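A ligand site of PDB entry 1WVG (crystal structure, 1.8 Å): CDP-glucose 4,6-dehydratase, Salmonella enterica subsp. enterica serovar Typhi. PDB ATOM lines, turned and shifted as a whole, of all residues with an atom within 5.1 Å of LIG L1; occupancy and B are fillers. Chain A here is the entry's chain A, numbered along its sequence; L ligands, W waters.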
ATOM      1  N   GLY A  16     -14.107   1.129   4.360  1.00  0.00           N
ATOM      2  CA  GLY A  16     -14.350   1.055   5.798  1.00  0.00           C
ATOM      3  C   GLY A  16     -15.667   1.689   6.261  1.00  0.00           C
ATOM      4  O   GLY A  16     -15.771   2.272   7.366  1.00  0.00           O
ATOM      5  N   HIS A  17     -16.713   1.531   5.441  1.00  0.00           N
ATOM      6  CA  HIS A  17     -18.049   2.106   5.751  1.00  0.00           C
ATOM      7  C   HIS A  17     -18.799   1.319   6.820  1.00  0.00           C
ATOM      8  O   HIS A  17     -19.764   1.809   7.424  1.00  0.00           O
ATOM      9  CB  HIS A  17     -18.906   2.216   4.465  1.00  0.00           C
ATOM     10  CG  HIS A  17     -19.181   0.849   3.942  1.00  0.00           C
ATOM     11  ND1 HIS A  17     -18.157  -0.001   3.539  1.00  0.00           N
ATOM     12  CD2 HIS A  17     -20.368   0.168   3.810  1.00  0.00           C
ATOM     13  CE1 HIS A  17     -18.716  -1.146   3.164  1.00  0.00           C
ATOM     14  NE2 HIS A  17     -20.044  -1.080   3.306  1.00  0.00           N
ATOM     15  N   THR A  18     -18.326   0.091   7.039  1.00  0.00           N
ATOM     16  CA  THR A  18     -18.974  -0.781   8.026  1.00  0.00           C
ATOM     17  C   THR A  18     -18.655  -0.477   9.483  1.00  0.00           C
ATOM     18  O   THR A  18     -19.290  -1.017  10.410  1.00  0.00           O
ATOM     19  CB  THR A  18     -18.741  -2.262   7.657  1.00  0.00           C
ATOM     20  OG1 THR A  18     -17.350  -2.522   7.710  1.00  0.00           O
ATOM     21  CG2 THR A  18     -19.210  -2.463   6.205  1.00  0.00           C
ATOM     22  N   GLY A  19     -17.666   0.376   9.703  1.00  0.00           N
ATOM     23  CA  GLY A  19     -17.247   0.723  11.024  1.00  0.00           C
ATOM     24  C   GLY A  19     -18.057   1.844  11.660  1.00  0.00           C
ATOM     25  O   GLY A  19     -19.089   2.315  11.158  1.00  0.00           O
ATOM     26  N   PHE A  20     -17.513   2.230  12.825  1.00  0.00           N
ATOM     27  CA  PHE A  20     -18.093   3.289  13.637  1.00  0.00           C
ATOM     28  C   PHE A  20     -18.109   4.613  12.894  1.00  0.00           C
ATOM     29  O   PHE A  20     -19.164   5.208  12.678  1.00  0.00           O
ATOM     30  CB  PHE A  20     -17.367   3.323  15.004  1.00  0.00           C
ATOM     31  CG  PHE A  20     -17.734   4.476  15.905  1.00  0.00           C
ATOM     32  CD1 PHE A  20     -19.046   4.643  16.358  1.00  0.00           C
ATOM     33  CD2 PHE A  20     -16.753   5.360  16.337  1.00  0.00           C
ATOM     34  CE1 PHE A  20     -19.394   5.679  17.213  1.00  0.00           C
ATOM     35  CE2 PHE A  20     -17.075   6.420  17.186  1.00  0.00           C
ATOM     36  CZ  PHE A  20     -18.383   6.555  17.643  1.00  0.00           C
ATOM     37  N   LYS A  21     -16.915   5.075  12.507  1.00  0.00           N
ATOM     38  CA  LYS A  21     -16.811   6.336  11.775  1.00  0.00           C
ATOM     39  C   LYS A  21     -17.557   6.242  10.450  1.00  0.00           C
ATOM     40  O   LYS A  21     -18.273   7.182  10.069  1.00  0.00           O
ATOM     41  CB  LYS A  21     -15.352   6.731  11.487  1.00  0.00           C
ATOM     42  CG  LYS A  21     -14.437   6.891  12.698  1.00  0.00           C
ATOM     43  CD  LYS A  21     -13.753   8.255  12.838  1.00  0.00           C
ATOM     44  CE  LYS A  21     -12.606   8.505  11.876  1.00  0.00           C
ATOM     45  NZ  LYS A  21     -11.357   8.995  12.504  1.00  0.00           N
ATOM     46  N   GLY A  22     -17.321   5.100   9.768  1.00  0.00           N
ATOM     47  CA  GLY A  22     -17.904   4.838   8.455  1.00  0.00           C
ATOM     48  C   GLY A  22     -19.398   4.928   8.413  1.00  0.00           C
ATOM     49  O   GLY A  22     -20.004   5.538   7.512  1.00  0.00           O
ATOM     50  N   TYR A  39     -16.904  -0.113   0.895  1.00  0.00           N
ATOM     51  CA  TYR A  39     -16.065  -1.264   0.629  1.00  0.00           C
ATOM     52  C   TYR A  39     -15.291  -1.484   1.885  1.00  0.00           C
ATOM     53  O   TYR A  39     -14.506  -0.629   2.285  1.00  0.00           O
ATOM     54  CB  TYR A  39     -15.121  -1.028  -0.584  1.00  0.00           C
ATOM     55  CG  TYR A  39     -14.143  -2.148  -0.937  1.00  0.00           C
ATOM     56  CD1 TYR A  39     -14.210  -2.812  -2.176  1.00  0.00           C
ATOM     57  CD2 TYR A  39     -13.095  -2.520  -0.093  1.00  0.00           C
ATOM     58  CE1 TYR A  39     -13.302  -3.810  -2.528  1.00  0.00           C
ATOM     59  CE2 TYR A  39     -12.151  -3.496  -0.454  1.00  0.00           C
ATOM     60  CZ  TYR A  39     -12.266  -4.170  -1.667  1.00  0.00           C
ATOM     61  OH  TYR A  39     -11.355  -5.148  -2.027  1.00  0.00           O
ATOM     62  N   ALA A  40     -15.582  -2.607   2.534  1.00  0.00           N
ATOM     63  CA  ALA A  40     -14.973  -2.970   3.794  1.00  0.00           C
ATOM     64  C   ALA A  40     -15.206  -4.450   4.087  1.00  0.00           C
ATOM     65  O   ALA A  40     -15.730  -5.215   3.285  1.00  0.00           O
ATOM     66  CB  ALA A  40     -15.678  -2.165   4.891  1.00  0.00           C
ATOM     67  N   LEU A  41     -14.808  -4.866   5.264  1.00  0.00           N
ATOM     68  CA  LEU A  41     -15.034  -6.239   5.646  1.00  0.00           C
ATOM     69  C   LEU A  41     -16.358  -6.251   6.376  1.00  0.00           C
ATOM     70  O   LEU A  41     -16.977  -5.181   6.496  1.00  0.00           O
ATOM     71  CB  LEU A  41     -13.874  -6.776   6.511  1.00  0.00           C
ATOM     72  CG  LEU A  41     -12.568  -6.717   5.763  1.00  0.00           C
ATOM     73  CD1 LEU A  41     -11.420  -6.833   6.729  1.00  0.00           C
ATOM     74  CD2 LEU A  41     -12.518  -7.818   4.725  1.00  0.00           C
ATOM     75  N   ASP A  42     -16.797  -7.397   6.859  1.00  0.00           N
ATOM     76  CA  ASP A  42     -18.048  -7.366   7.579  1.00  0.00           C
ATOM     77  C   ASP A  42     -17.881  -6.556   8.870  1.00  0.00           C
ATOM     78  O   ASP A  42     -16.751  -6.474   9.391  1.00  0.00           O
ATOM     79  CB  ASP A  42     -18.672  -8.769   7.809  1.00  0.00           C
ATOM     80  CG  ASP A  42     -19.622  -9.216   6.716  1.00  0.00           C
ATOM     81  OD1 ASP A  42     -20.787  -8.870   6.650  1.00  0.00           O
ATOM     82  OD2 ASP A  42     -19.083 -10.033   5.848  1.00  0.00           O
ATOM     83  N   PRO A  44     -17.143  -4.692  11.988  1.00  0.00           N
ATOM     84  CA  PRO A  44     -16.069  -4.930  12.898  1.00  0.00           C
ATOM     85  C   PRO A  44     -16.537  -5.546  14.182  1.00  0.00           C
ATOM     86  O   PRO A  44     -15.768  -6.255  14.806  1.00  0.00           O
ATOM     87  CB  PRO A  44     -15.430  -3.562  13.172  1.00  0.00           C
ATOM     88  CG  PRO A  44     -16.411  -2.513  12.667  1.00  0.00           C
ATOM     89  CD  PRO A  44     -17.452  -3.232  11.843  1.00  0.00           C
ATOM     90  N   GLY A  64     -15.479  -6.515   1.039  1.00  0.00           N
ATOM     91  CA  GLY A  64     -14.217  -6.865   0.404  1.00  0.00           C
ATOM     92  C   GLY A  64     -12.990  -6.399   1.186  1.00  0.00           C
ATOM     93  O   GLY A  64     -13.079  -5.603   2.115  1.00  0.00           O
ATOM     94  N   ASP A  65     -11.837  -6.931   0.776  1.00  0.00           N
ATOM     95  CA  ASP A  65     -10.605  -6.626   1.446  1.00  0.00           C
ATOM     96  C   ASP A  65      -9.764  -5.595   0.737  1.00  0.00           C
ATOM     97  O   ASP A  65      -9.486  -5.699  -0.474  1.00  0.00           O
ATOM     98  CB  ASP A  65      -9.753  -7.868   1.602  1.00  0.00           C
ATOM     99  CG  ASP A  65      -8.745  -7.599   2.647  1.00  0.00           C
ATOM    100  OD1 ASP A  65      -8.003  -6.618   2.695  1.00  0.00           O
ATOM    101  OD2 ASP A  65      -8.785  -8.554   3.521  1.00  0.00           O
ATOM    102  N   ILE A  66      -9.366  -4.621   1.563  1.00  0.00           N
ATOM    103  CA  ILE A  66      -8.550  -3.551   1.019  1.00  0.00           C
ATOM    104  C   ILE A  66      -7.201  -4.032   0.461  1.00  0.00           C
ATOM    105  O   ILE A  66      -6.543  -3.411  -0.375  1.00  0.00           O
ATOM    106  CB  ILE A  66      -8.395  -2.441   2.038  1.00  0.00           C
ATOM    107  CG1 ILE A  66      -8.023  -1.158   1.300  1.00  0.00           C
ATOM    108  CG2 ILE A  66      -7.348  -2.814   3.076  1.00  0.00           C
ATOM    109  CD1 ILE A  66      -9.236  -0.573   0.580  1.00  0.00           C
ATOM    110  N   ARG A  67      -6.783  -5.178   0.938  1.00  0.00           N
ATOM    111  CA  ARG A  67      -5.549  -5.738   0.473  1.00  0.00           C
ATOM    112  C   ARG A  67      -5.663  -6.414  -0.880  1.00  0.00           C
ATOM    113  O   ARG A  67      -4.680  -6.848  -1.471  1.00  0.00           O
ATOM    114  CB  ARG A  67      -4.981  -6.669   1.531  1.00  0.00           C
ATOM    115  CG  ARG A  67      -4.656  -5.889   2.792  1.00  0.00           C
ATOM    116  CD  ARG A  67      -4.382  -6.811   3.967  1.00  0.00           C
ATOM    117  NE  ARG A  67      -5.614  -7.324   4.511  1.00  0.00           N
ATOM    118  CZ  ARG A  67      -5.711  -8.228   5.489  1.00  0.00           C
ATOM    119  NH1 ARG A  67      -4.635  -8.758   6.084  1.00  0.00           N
ATOM    120  NH2 ARG A  67      -6.929  -8.622   5.885  1.00  0.00           N
ATOM    121  N   MET A  87     -11.250   5.132   4.778  1.00  0.00           N
ATOM    122  CA  MET A  87     -11.276   4.885   6.230  1.00  0.00           C
ATOM    123  C   MET A  87     -11.086   3.439   6.677  1.00  0.00           C
ATOM    124  O   MET A  87     -11.163   3.169   7.875  1.00  0.00           O
ATOM    125  CB  MET A  87     -12.601   5.325   6.848  1.00  0.00           C
ATOM    126  CG  MET A  87     -12.843   6.811   6.662  1.00  0.00           C
ATOM    127  SD  MET A  87     -14.200   7.452   7.687  1.00  0.00           S
ATOM    128  CE  MET A  87     -15.555   7.306   6.496  1.00  0.00           C
ATOM    129  N   ALA A  88     -10.870   2.514   5.758  1.00  0.00           N
ATOM    130  CA  ALA A  88     -10.714   1.140   6.185  1.00  0.00           C
ATOM    131  C   ALA A  88      -9.392   0.972   6.899  1.00  0.00           C
ATOM    132  O   ALA A  88      -8.374   1.427   6.380  1.00  0.00           O
ATOM    133  CB  ALA A  88     -10.764   0.199   4.994  1.00  0.00           C
ATOM    134  N   ALA A  89      -9.380   0.349   8.064  1.00  0.00           N
ATOM    135  CA  ALA A  89      -8.148   0.131   8.803  1.00  0.00           C
ATOM    136  C   ALA A  89      -8.399  -0.776  10.007  1.00  0.00           C
ATOM    137  O   ALA A  89      -9.561  -0.938  10.430  1.00  0.00           O
ATOM    138  CB  ALA A  89      -7.643   1.467   9.345  1.00  0.00           C
ATOM    139  N   GLN A  90      -7.281  -1.343  10.506  1.00  0.00           N
ATOM    140  CA  GLN A  90      -7.161  -2.113  11.728  1.00  0.00           C
ATOM    141  C   GLN A  90      -6.811  -0.913  12.627  1.00  0.00           C
ATOM    142  O   GLN A  90      -5.649  -0.422  12.588  1.00  0.00           O
ATOM    143  CB  GLN A  90      -6.029  -3.141  11.570  1.00  0.00           C
ATOM    144  CG  GLN A  90      -5.873  -4.066  12.809  1.00  0.00           C
ATOM    145  CD  GLN A  90      -5.802  -3.316  14.145  1.00  0.00           C
ATOM    146  OE1 GLN A  90      -6.826  -2.951  14.676  1.00  0.00           O
ATOM    147  NE2 GLN A  90      -4.608  -3.131  14.735  1.00  0.00           N
ATOM    148  N   PRO A  91      -7.820  -0.324  13.338  1.00  0.00           N
ATOM    149  CA  PRO A  91      -7.539   0.893  14.082  1.00  0.00           C
ATOM    150  C   PRO A  91      -7.105   0.762  15.538  1.00  0.00           C
ATOM    151  O   PRO A  91      -6.942   1.765  16.226  1.00  0.00           O
ATOM    152  CB  PRO A  91      -8.884   1.615  14.085  1.00  0.00           C
ATOM    153  CG  PRO A  91      -9.899   0.508  14.233  1.00  0.00           C
ATOM    154  CD  PRO A  91      -9.248  -0.705  13.585  1.00  0.00           C
ATOM    155  N   LYS A 102      -0.800  -7.845  10.060  1.00  0.00           N
ATOM    156  CA  LYS A 102      -2.090  -7.499   9.513  1.00  0.00           C
ATOM    157  C   LYS A 102      -2.319  -5.993   9.626  1.00  0.00           C
ATOM    158  O   LYS A 102      -3.035  -5.359   8.822  1.00  0.00           O
ATOM    159  CB  LYS A 102      -3.137  -8.193  10.359  1.00  0.00           C
ATOM    160  CG  LYS A 102      -4.514  -8.213   9.732  1.00  0.00           C
ATOM    161  CD  LYS A 102      -5.495  -7.141  10.218  1.00  0.00           C
ATOM    162  CE  LYS A 102      -6.450  -6.735   9.088  1.00  0.00           C
ATOM    163  NZ  LYS A 102      -7.526  -5.772   9.398  1.00  0.00           N
ATOM    164  N   THR A 106      -2.832  -3.951   6.242  1.00  0.00           N
ATOM    165  CA  THR A 106      -4.089  -3.254   6.092  1.00  0.00           C
ATOM    166  C   THR A 106      -3.925  -1.743   5.915  1.00  0.00           C
ATOM    167  O   THR A 106      -4.425  -1.138   4.975  1.00  0.00           O
ATOM    168  CB  THR A 106      -5.067  -3.510   7.261  1.00  0.00           C
ATOM    169  OG1 THR A 106      -5.349  -4.891   7.340  1.00  0.00           O
ATOM    170  CG2 THR A 106      -6.386  -2.761   7.034  1.00  0.00           C
ATOM    171  N   ILE A 130      -8.138   9.303   5.571  1.00  0.00           N
ATOM    172  CA  ILE A 130      -8.202   9.336   7.005  1.00  0.00           C
ATOM    173  C   ILE A 130      -7.027   8.621   7.654  1.00  0.00           C
ATOM    174  O   ILE A 130      -6.844   7.410   7.496  1.00  0.00           O
ATOM    175  CB  ILE A 130      -9.470   8.668   7.526  1.00  0.00           C
ATOM    176  CG1 ILE A 130     -10.658   9.608   7.347  1.00  0.00           C
ATOM    177  CG2 ILE A 130      -9.244   8.363   9.008  1.00  0.00           C
ATOM    178  CD1 ILE A 130     -10.970   9.903   5.905  1.00  0.00           C
ATOM    179  N   THR A 131      -6.202   9.372   8.388  1.00  0.00           N
ATOM    180  CA  THR A 131      -5.079   8.723   9.034  1.00  0.00           C
ATOM    181  C   THR A 131      -5.392   8.581  10.530  1.00  0.00           C
ATOM    182  O   THR A 131      -6.326   7.874  10.915  1.00  0.00           O
ATOM    183  CB  THR A 131      -3.692   9.328   8.686  1.00  0.00           C
ATOM    184  OG1 THR A 131      -3.642  10.677   9.125  1.00  0.00           O
ATOM    185  CG2 THR A 131      -3.472   9.277   7.182  1.00  0.00           C
ATOM    186  N   TYR A 157       0.232   0.108  15.258  1.00  0.00           N
ATOM    187  CA  TYR A 157      -0.902   0.875  14.763  1.00  0.00           C
ATOM    188  C   TYR A 157      -0.484   2.354  14.522  1.00  0.00           C
ATOM    189  O   TYR A 157      -0.601   2.868  13.410  1.00  0.00           O
ATOM    190  CB  TYR A 157      -2.082   0.831  15.737  1.00  0.00           C
ATOM    191  CG  TYR A 157      -3.061   1.875  15.295  1.00  0.00           C
ATOM    192  CD1 TYR A 157      -3.772   1.691  14.114  1.00  0.00           C
ATOM    193  CD2 TYR A 157      -3.278   3.028  16.046  1.00  0.00           C
ATOM    194  CE1 TYR A 157      -4.710   2.640  13.696  1.00  0.00           C
ATOM    195  CE2 TYR A 157      -4.187   4.001  15.632  1.00  0.00           C
ATOM    196  CZ  TYR A 157      -4.904   3.808  14.441  1.00  0.00           C
ATOM    197  OH  TYR A 157      -5.817   4.741  14.012  1.00  0.00           O
ATOM    198  N   LYS A 161       0.117   4.418  10.679  1.00  0.00           N
ATOM    199  CA  LYS A 161      -0.570   5.691  10.308  1.00  0.00           C
ATOM    200  C   LYS A 161       0.426   6.770   9.851  1.00  0.00           C
ATOM    201  O   LYS A 161       0.214   7.607   8.941  1.00  0.00           O
ATOM    202  CB  LYS A 161      -1.441   6.164  11.466  1.00  0.00           C
ATOM    203  CG  LYS A 161      -2.611   5.221  11.652  1.00  0.00           C
ATOM    204  CD  LYS A 161      -3.517   5.257  10.425  1.00  0.00           C
ATOM    205  CE  LYS A 161      -4.711   4.362  10.605  1.00  0.00           C
ATOM    206  NZ  LYS A 161      -5.880   4.872   9.901  1.00  0.00           N
ATOM    207  N   VAL A 196     -12.384   9.910  18.682  1.00  0.00           N
ATOM    208  CA  VAL A 196     -13.822  10.015  18.494  1.00  0.00           C
ATOM    209  C   VAL A 196     -14.567   9.139  19.461  1.00  0.00           C
ATOM    210  O   VAL A 196     -14.243   7.964  19.634  1.00  0.00           O
ATOM    211  CB  VAL A 196     -14.331   9.603  17.098  1.00  0.00           C
ATOM    212  CG1 VAL A 196     -14.007  10.676  16.087  1.00  0.00           C
ATOM    213  CG2 VAL A 196     -13.741   8.270  16.647  1.00  0.00           C
ATOM    214  N   ASP A 201     -20.391   2.870  19.203  1.00  0.00           N
ATOM    215  CA  ASP A 201     -19.056   2.295  19.055  1.00  0.00           C
ATOM    216  C   ASP A 201     -18.814   1.128  19.967  1.00  0.00           C
ATOM    217  O   ASP A 201     -18.845   1.267  21.224  1.00  0.00           O
ATOM    218  CB  ASP A 201     -17.900   3.301  19.271  1.00  0.00           C
ATOM    219  CG  ASP A 201     -16.510   2.774  18.927  1.00  0.00           C
ATOM    220  OD1 ASP A 201     -15.498   3.308  19.346  1.00  0.00           O
ATOM    221  OD2 ASP A 201     -16.481   1.717  18.118  1.00  0.00           O
ATOM    222  N   ARG A 206     -11.587   0.288  23.755  1.00  0.00           N
ATOM    223  CA  ARG A 206     -11.741   1.730  23.735  1.00  0.00           C
ATOM    224  C   ARG A 206     -12.406   2.119  25.021  1.00  0.00           C
ATOM    225  O   ARG A 206     -13.163   1.334  25.567  1.00  0.00           O
ATOM    226  CB  ARG A 206     -12.426   2.279  22.477  1.00  0.00           C
ATOM    227  CG  ARG A 206     -11.621   2.039  21.174  1.00  0.00           C
ATOM    228  CD  ARG A 206     -12.173   2.918  20.049  1.00  0.00           C
ATOM    229  NE  ARG A 206     -11.455   2.823  18.801  1.00  0.00           N
ATOM    230  CZ  ARG A 206     -12.007   2.971  17.593  1.00  0.00           C
ATOM    231  NH1 ARG A 206     -13.307   3.225  17.411  1.00  0.00           N
ATOM    232  NH2 ARG A 206     -11.249   2.876  16.502  1.00  0.00           N
HETATM  233  N1  LIG L   1     -10.296  -4.396   4.174  1.00  0.00           N
HETATM  234  C1  LIG L   1     -11.397  -3.604   4.165  1.00  0.00           C
HETATM  235  N2  LIG L   1     -11.956  -2.987   5.160  1.00  0.00           N
HETATM  236  C2  LIG L   1     -11.277  -3.165   6.316  1.00  0.00           C
HETATM  237  C3  LIG L   1     -10.159  -3.899   6.500  1.00  0.00           C
HETATM  238  C4  LIG L   1      -9.640  -4.581   5.360  1.00  0.00           C
HETATM  239  N3  LIG L   1      -8.525  -5.330   5.294  1.00  0.00           N
HETATM  240  N4  LIG L   1      -9.744  -3.841   7.820  1.00  0.00           N
HETATM  241  C5  LIG L   1     -10.644  -3.067   8.413  1.00  0.00           C
HETATM  242  N5  LIG L   1     -11.600  -2.635   7.545  1.00  0.00           N
HETATM  243  C6  LIG L   1     -12.757  -1.802   7.788  1.00  0.00           C
HETATM  244  C7  LIG L   1     -13.708  -2.467   8.744  1.00  0.00           C
HETATM  245  O1  LIG L   1     -14.443  -3.495   8.074  1.00  0.00           O
HETATM  246  C8  LIG L   1     -14.572  -1.253   9.104  1.00  0.00           C
HETATM  247  O2  LIG L   1     -15.547  -0.841   8.143  1.00  0.00           O
HETATM  248  O3  LIG L   1     -12.352  -0.666   8.476  1.00  0.00           O
HETATM  249  C9  LIG L   1     -13.448  -0.183   9.255  1.00  0.00           C
HETATM  250  C10 LIG L   1     -12.899  -0.040  10.637  1.00  0.00           C
HETATM  251  O4  LIG L   1     -13.933   0.549  11.453  1.00  0.00           O
HETATM  252  P1  LIG L   1     -13.853   0.533  13.086  1.00  0.00           P
HETATM  253  O5  LIG L   1     -13.081  -0.659  13.622  1.00  0.00           O
HETATM  254  O6  LIG L   1     -15.257   0.895  13.634  1.00  0.00           O
HETATM  255  O7  LIG L   1     -12.918   1.771  13.352  1.00  0.00           O
HETATM  256  P2  LIG L   1     -13.310   3.342  13.265  1.00  0.00           P
HETATM  257  O8  LIG L   1     -13.309   3.847  14.686  1.00  0.00           O
HETATM  258  O9  LIG L   1     -14.519   3.584  12.373  1.00  0.00           O
HETATM  259  O10 LIG L   1     -12.080   3.865  12.402  1.00  0.00           O
HETATM  260  C11 LIG L   1     -12.343   4.408  11.099  1.00  0.00           C
HETATM  261  O11 LIG L   1     -10.708   6.261  11.308  1.00  0.00           O
HETATM  262  O12 LIG L   1      -9.581   6.605  13.331  1.00  0.00           O
HETATM  263  C12 LIG L   1      -9.484   6.091  11.971  1.00  0.00           C
HETATM  264  O13 LIG L   1      -7.895   4.224  12.002  1.00  0.00           O
HETATM  265  C13 LIG L   1      -9.292   4.595  12.034  1.00  0.00           C
HETATM  266  O14 LIG L   1      -8.879   4.388   9.696  1.00  0.00           O
HETATM  267  C14 LIG L   1      -9.852   4.141  10.703  1.00  0.00           C
HETATM  268  C15 LIG L   1     -11.069   5.032  10.591  1.00  0.00           C
HETATM  269  O1  LG2 L   2      -6.244   6.485  22.005  1.00  0.00           O
HETATM  270  P1  LG2 L   2      -6.674   5.115  21.537  1.00  0.00           P
HETATM  271  O2  LG2 L   2      -5.694   4.014  21.874  1.00  0.00           O
HETATM  272  O3  LG2 L   2      -6.947   5.141  19.911  1.00  0.00           O
HETATM  273  O4  LG2 L   2      -8.023   5.066  22.281  1.00  0.00           O
HETATM  274  P2  LG2 L   2      -8.547   4.175  23.564  1.00  0.00           P
HETATM  275  O5  LG2 L   2      -9.974   4.555  23.737  1.00  0.00           O
HETATM  276  O6  LG2 L   2      -8.318   2.728  23.331  1.00  0.00           O
HETATM  277  O7  LG2 L   2      -7.578   4.686  24.725  1.00  0.00           O
HETATM  278  C1  LG2 L   2      -7.834   5.985  25.287  1.00  0.00           C
HETATM  279  C2  LG2 L   2      -7.066   6.096  26.575  1.00  0.00           C
HETATM  280  O8  LG2 L   2      -7.890   5.526  27.629  1.00  0.00           O
HETATM  281  C3  LG2 L   2      -5.694   5.435  26.658  1.00  0.00           C
HETATM  282  O9  LG2 L   2      -4.692   6.134  27.481  1.00  0.00           O
HETATM  283  C4  LG2 L   2      -6.127   4.092  27.279  1.00  0.00           C
HETATM  284  O10 LG2 L   2      -4.998   3.494  27.909  1.00  0.00           O
HETATM  285  C5  LG2 L   2      -7.120   4.585  28.313  1.00  0.00           C
HETATM  286  N1  LG2 L   2      -8.017   3.540  28.804  1.00  0.00           N
HETATM  287  C6  LG2 L   2      -8.875   2.878  27.934  1.00  0.00           C
HETATM  288  C7  LG2 L   2      -9.714   1.958  28.327  1.00  0.00           C
HETATM  289  C8  LG2 L   2      -9.783   1.552  29.684  1.00  0.00           C
HETATM  290  N2  LG2 L   2      -8.914   2.265  30.525  1.00  0.00           N
HETATM  291  C9  LG2 L   2      -8.010   3.239  30.150  1.00  0.00           C
HETATM  292  N3  LG2 L   2     -10.511   0.672  30.140  1.00  0.00           N
HETATM  293  O11 LG2 L   2      -7.259   3.809  30.946  1.00  0.00           O
HETATM  294  C10 LG2 L   2      -8.248   5.571  19.563  1.00  0.00           C
HETATM  295  C11 LG2 L   2      -8.663   4.716  18.397  1.00  0.00           C
HETATM  296  C12 LG2 L   2      -7.682   4.988  17.284  1.00  0.00           C
HETATM  297  C13 LG2 L   2      -7.691   6.475  16.907  1.00  0.00           C
HETATM  298  C14 LG2 L   2      -7.403   7.318  18.148  1.00  0.00           C
HETATM  299  O12 LG2 L   2      -8.618   3.306  18.709  1.00  0.00           O
HETATM  300  O13 LG2 L   2      -8.071   4.261  16.107  1.00  0.00           O
HETATM  301  O14 LG2 L   2      -6.746   6.731  15.879  1.00  0.00           O
HETATM  302  O15 LG2 L   2      -8.310   6.988  19.205  1.00  0.00           O
HETATM  303  O   HOH W   1      -7.672   4.562   6.983  1.00  0.00           O
HETATM  304  O   HOH W   2     -15.808   3.005   9.974  1.00  0.00           O
HETATM  305  O   HOH W   3     -14.299  -5.431   9.793  1.00  0.00           O
HETATM  306  O   HOH W   4      -8.663   9.290  13.057  1.00  0.00           O
HETATM  307  O   HOH W   5     -11.500  -3.188  12.984  1.00  0.00           O
HETATM  308  O   HOH W   6     -13.771  -2.028  16.146  1.00  0.00           O
HETATM  309  O   HOH W   7     -15.917   0.128  16.198  1.00  0.00           O
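An oxygen (O2) of LIG L1 lies within hydrogen-bond range of the backbone NH (N) of Thr 18, 3.1 Å away.
The side-chain hydroxyl (OG1) of Thr 18 sits at hydrogen-bond distance from an oxygen (O2) of LIG L1, at 2.5 Å.
An oxygen (O6) of LIG L1 sits at hydrogen-bond distance from the backbone NH of Phe 20 (2.7 Å).
N1 of LIG L1 sits at hydrogen-bond distance from N of Ile 66, at 2.8 Å.
NH1 of Arg 206 is in salt-bridge range of O8 of LIG L1.
The backbone NH of Lys 21 lies within hydrogen-bond range of an oxygen (O9) of LIG L1.
An oxygen (O11) of LIG L1 lies close to the side-chain amino group (NZ) of Lys 21 (3.1 Å).
An oxygen (O2) of LIG L1 sits at hydrogen-bond distance from the backbone NH (N) of Gly 19 (2.9 Å).
The side-chain hydroxyl (OH) of Tyr 157 sits at hydrogen-bond distance from an oxygen (O13) of LIG L1 (2.9 Å).
OD1 of Asp 65 sits at hydrogen-bond distance from N3 of LIG L1 (2.9 Å).
An oxygen (O13) of LIG L1 lies within hydrogen-bond range of the side-chain amino group (NZ) of Lys 161, 3.0 Å away.
The backbone NH (N) of Ala 89 lies within hydrogen-bond range of an oxygen (O3) of LIG L1 (3.2 Å).
N of Leu 41 lies within hydrogen-bond range of O1 of LIG L1.
O of Leu 41 lies within hydrogen-bond range of O1 of LIG L1 (3.4 Å).
O2 of LIG L1 lies close to O of Gly 16, at 3.2 Å.
O of Met 87 sits at hydrogen-bond distance from O14 of LIG L1 (3.2 Å).
A nitrogen (N4) of LIG L1 is in hydrogen-bond range of the side-chain amino group of Lys 102, 3.3 Å away.
O12 of LG2 L2 lies within hydrogen-bond range of NE of Arg 206, 2.9 Å away.
The side-chain hydroxyl (OH) of Tyr 157 lies within hydrogen-bond range of an oxygen (O14) of LG2 L2, 2.9 Å away.
O13 of LG2 L2 sits at hydrogen-bond distance from O of Pro 91.
The side-chain hydroxyl (OG1) of Thr 18 is in hydrogen-bond range of the backbone carbonyl oxygen (O) of Leu 41 (2.9 Å).
NH2 of Arg 67 is in salt-bridge range of OD2 of Asp 65 (3.0 Å).
The backbone carbonyl oxygen of Asp 65 lies within hydrogen-bond range of the side-chain hydroxyl of Tyr 39 (2.5 Å).
NZ of Lys 161 sits at hydrogen-bond distance from O of Thr 131, at 3.2 Å.
N of Gly 16 sits at hydrogen-bond distance from O of Tyr 39 (2.7 Å).
The backbone carbonyl oxygen of Ala 40 lies within hydrogen-bond range of the backbone NH of Gly 64 (2.6 Å).
The backbone carbonyl oxygen of Lys 102 sits close to the side-chain hydroxyl of Thr 106 (2.8 Å).
N of Tyr 39 sits at hydrogen-bond distance from ND1 of His 17.
His 17 touches LIG L1 (N to O2, 3.8 Å).
CA of Ala 40 touches N2 of LIG L1, 3.3 Å away.
Asp 42 touches LIG L1.
CG of Pro 44 touches O6 of LIG L1 (3.7 Å).
Gly 64 touches LIG L1.
Arg 67 touches LIG L1.
Ala 88 touches LIG L1 (CA to O3, 3.3 Å).
Pro 91 touches LIG L1 (CG to O7, 3.4 Å).
Thr 106 touches LIG L1.
CG2 of Ile 130 touches O11 of LIG L1, 3.4 Å away.
O of Thr 131 touches C12 of LIG L1, 3.8 Å away.
Hydrophobic or aromatic side chains that line LIG L1: Phe 20, Ala 40, Leu 41, Pro 44, Ile 66, Ala 88, Ala 89, Pro 91, Ile 130 and Tyr 157.
The nearest printed residue that does not touch LIG L1 is Gly 22 (4.1 Å).
Water W3 lies within hydrogen-bond range of O1 of LIG L1 (2.6 Å) and O of Asp 42 (2.7 Å).
Water W7 bridges the side-chain carboxylate (OD2) of Asp 201 and an oxygen (O6) of LIG L1.
Water W4 lies within hydrogen-bond range of the side-chain amino group (NZ) of Lys 21 (2.8 Å), an oxygen (O12) of LIG L1 (2.9 Å) and the backbone carbonyl oxygen (O) of Thr 131 (3.5 Å).
Water W1 lies within hydrogen-bond range of O14 of LIG L1, O of Ile 130, O of Ala 88 and NZ of Lys 161.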
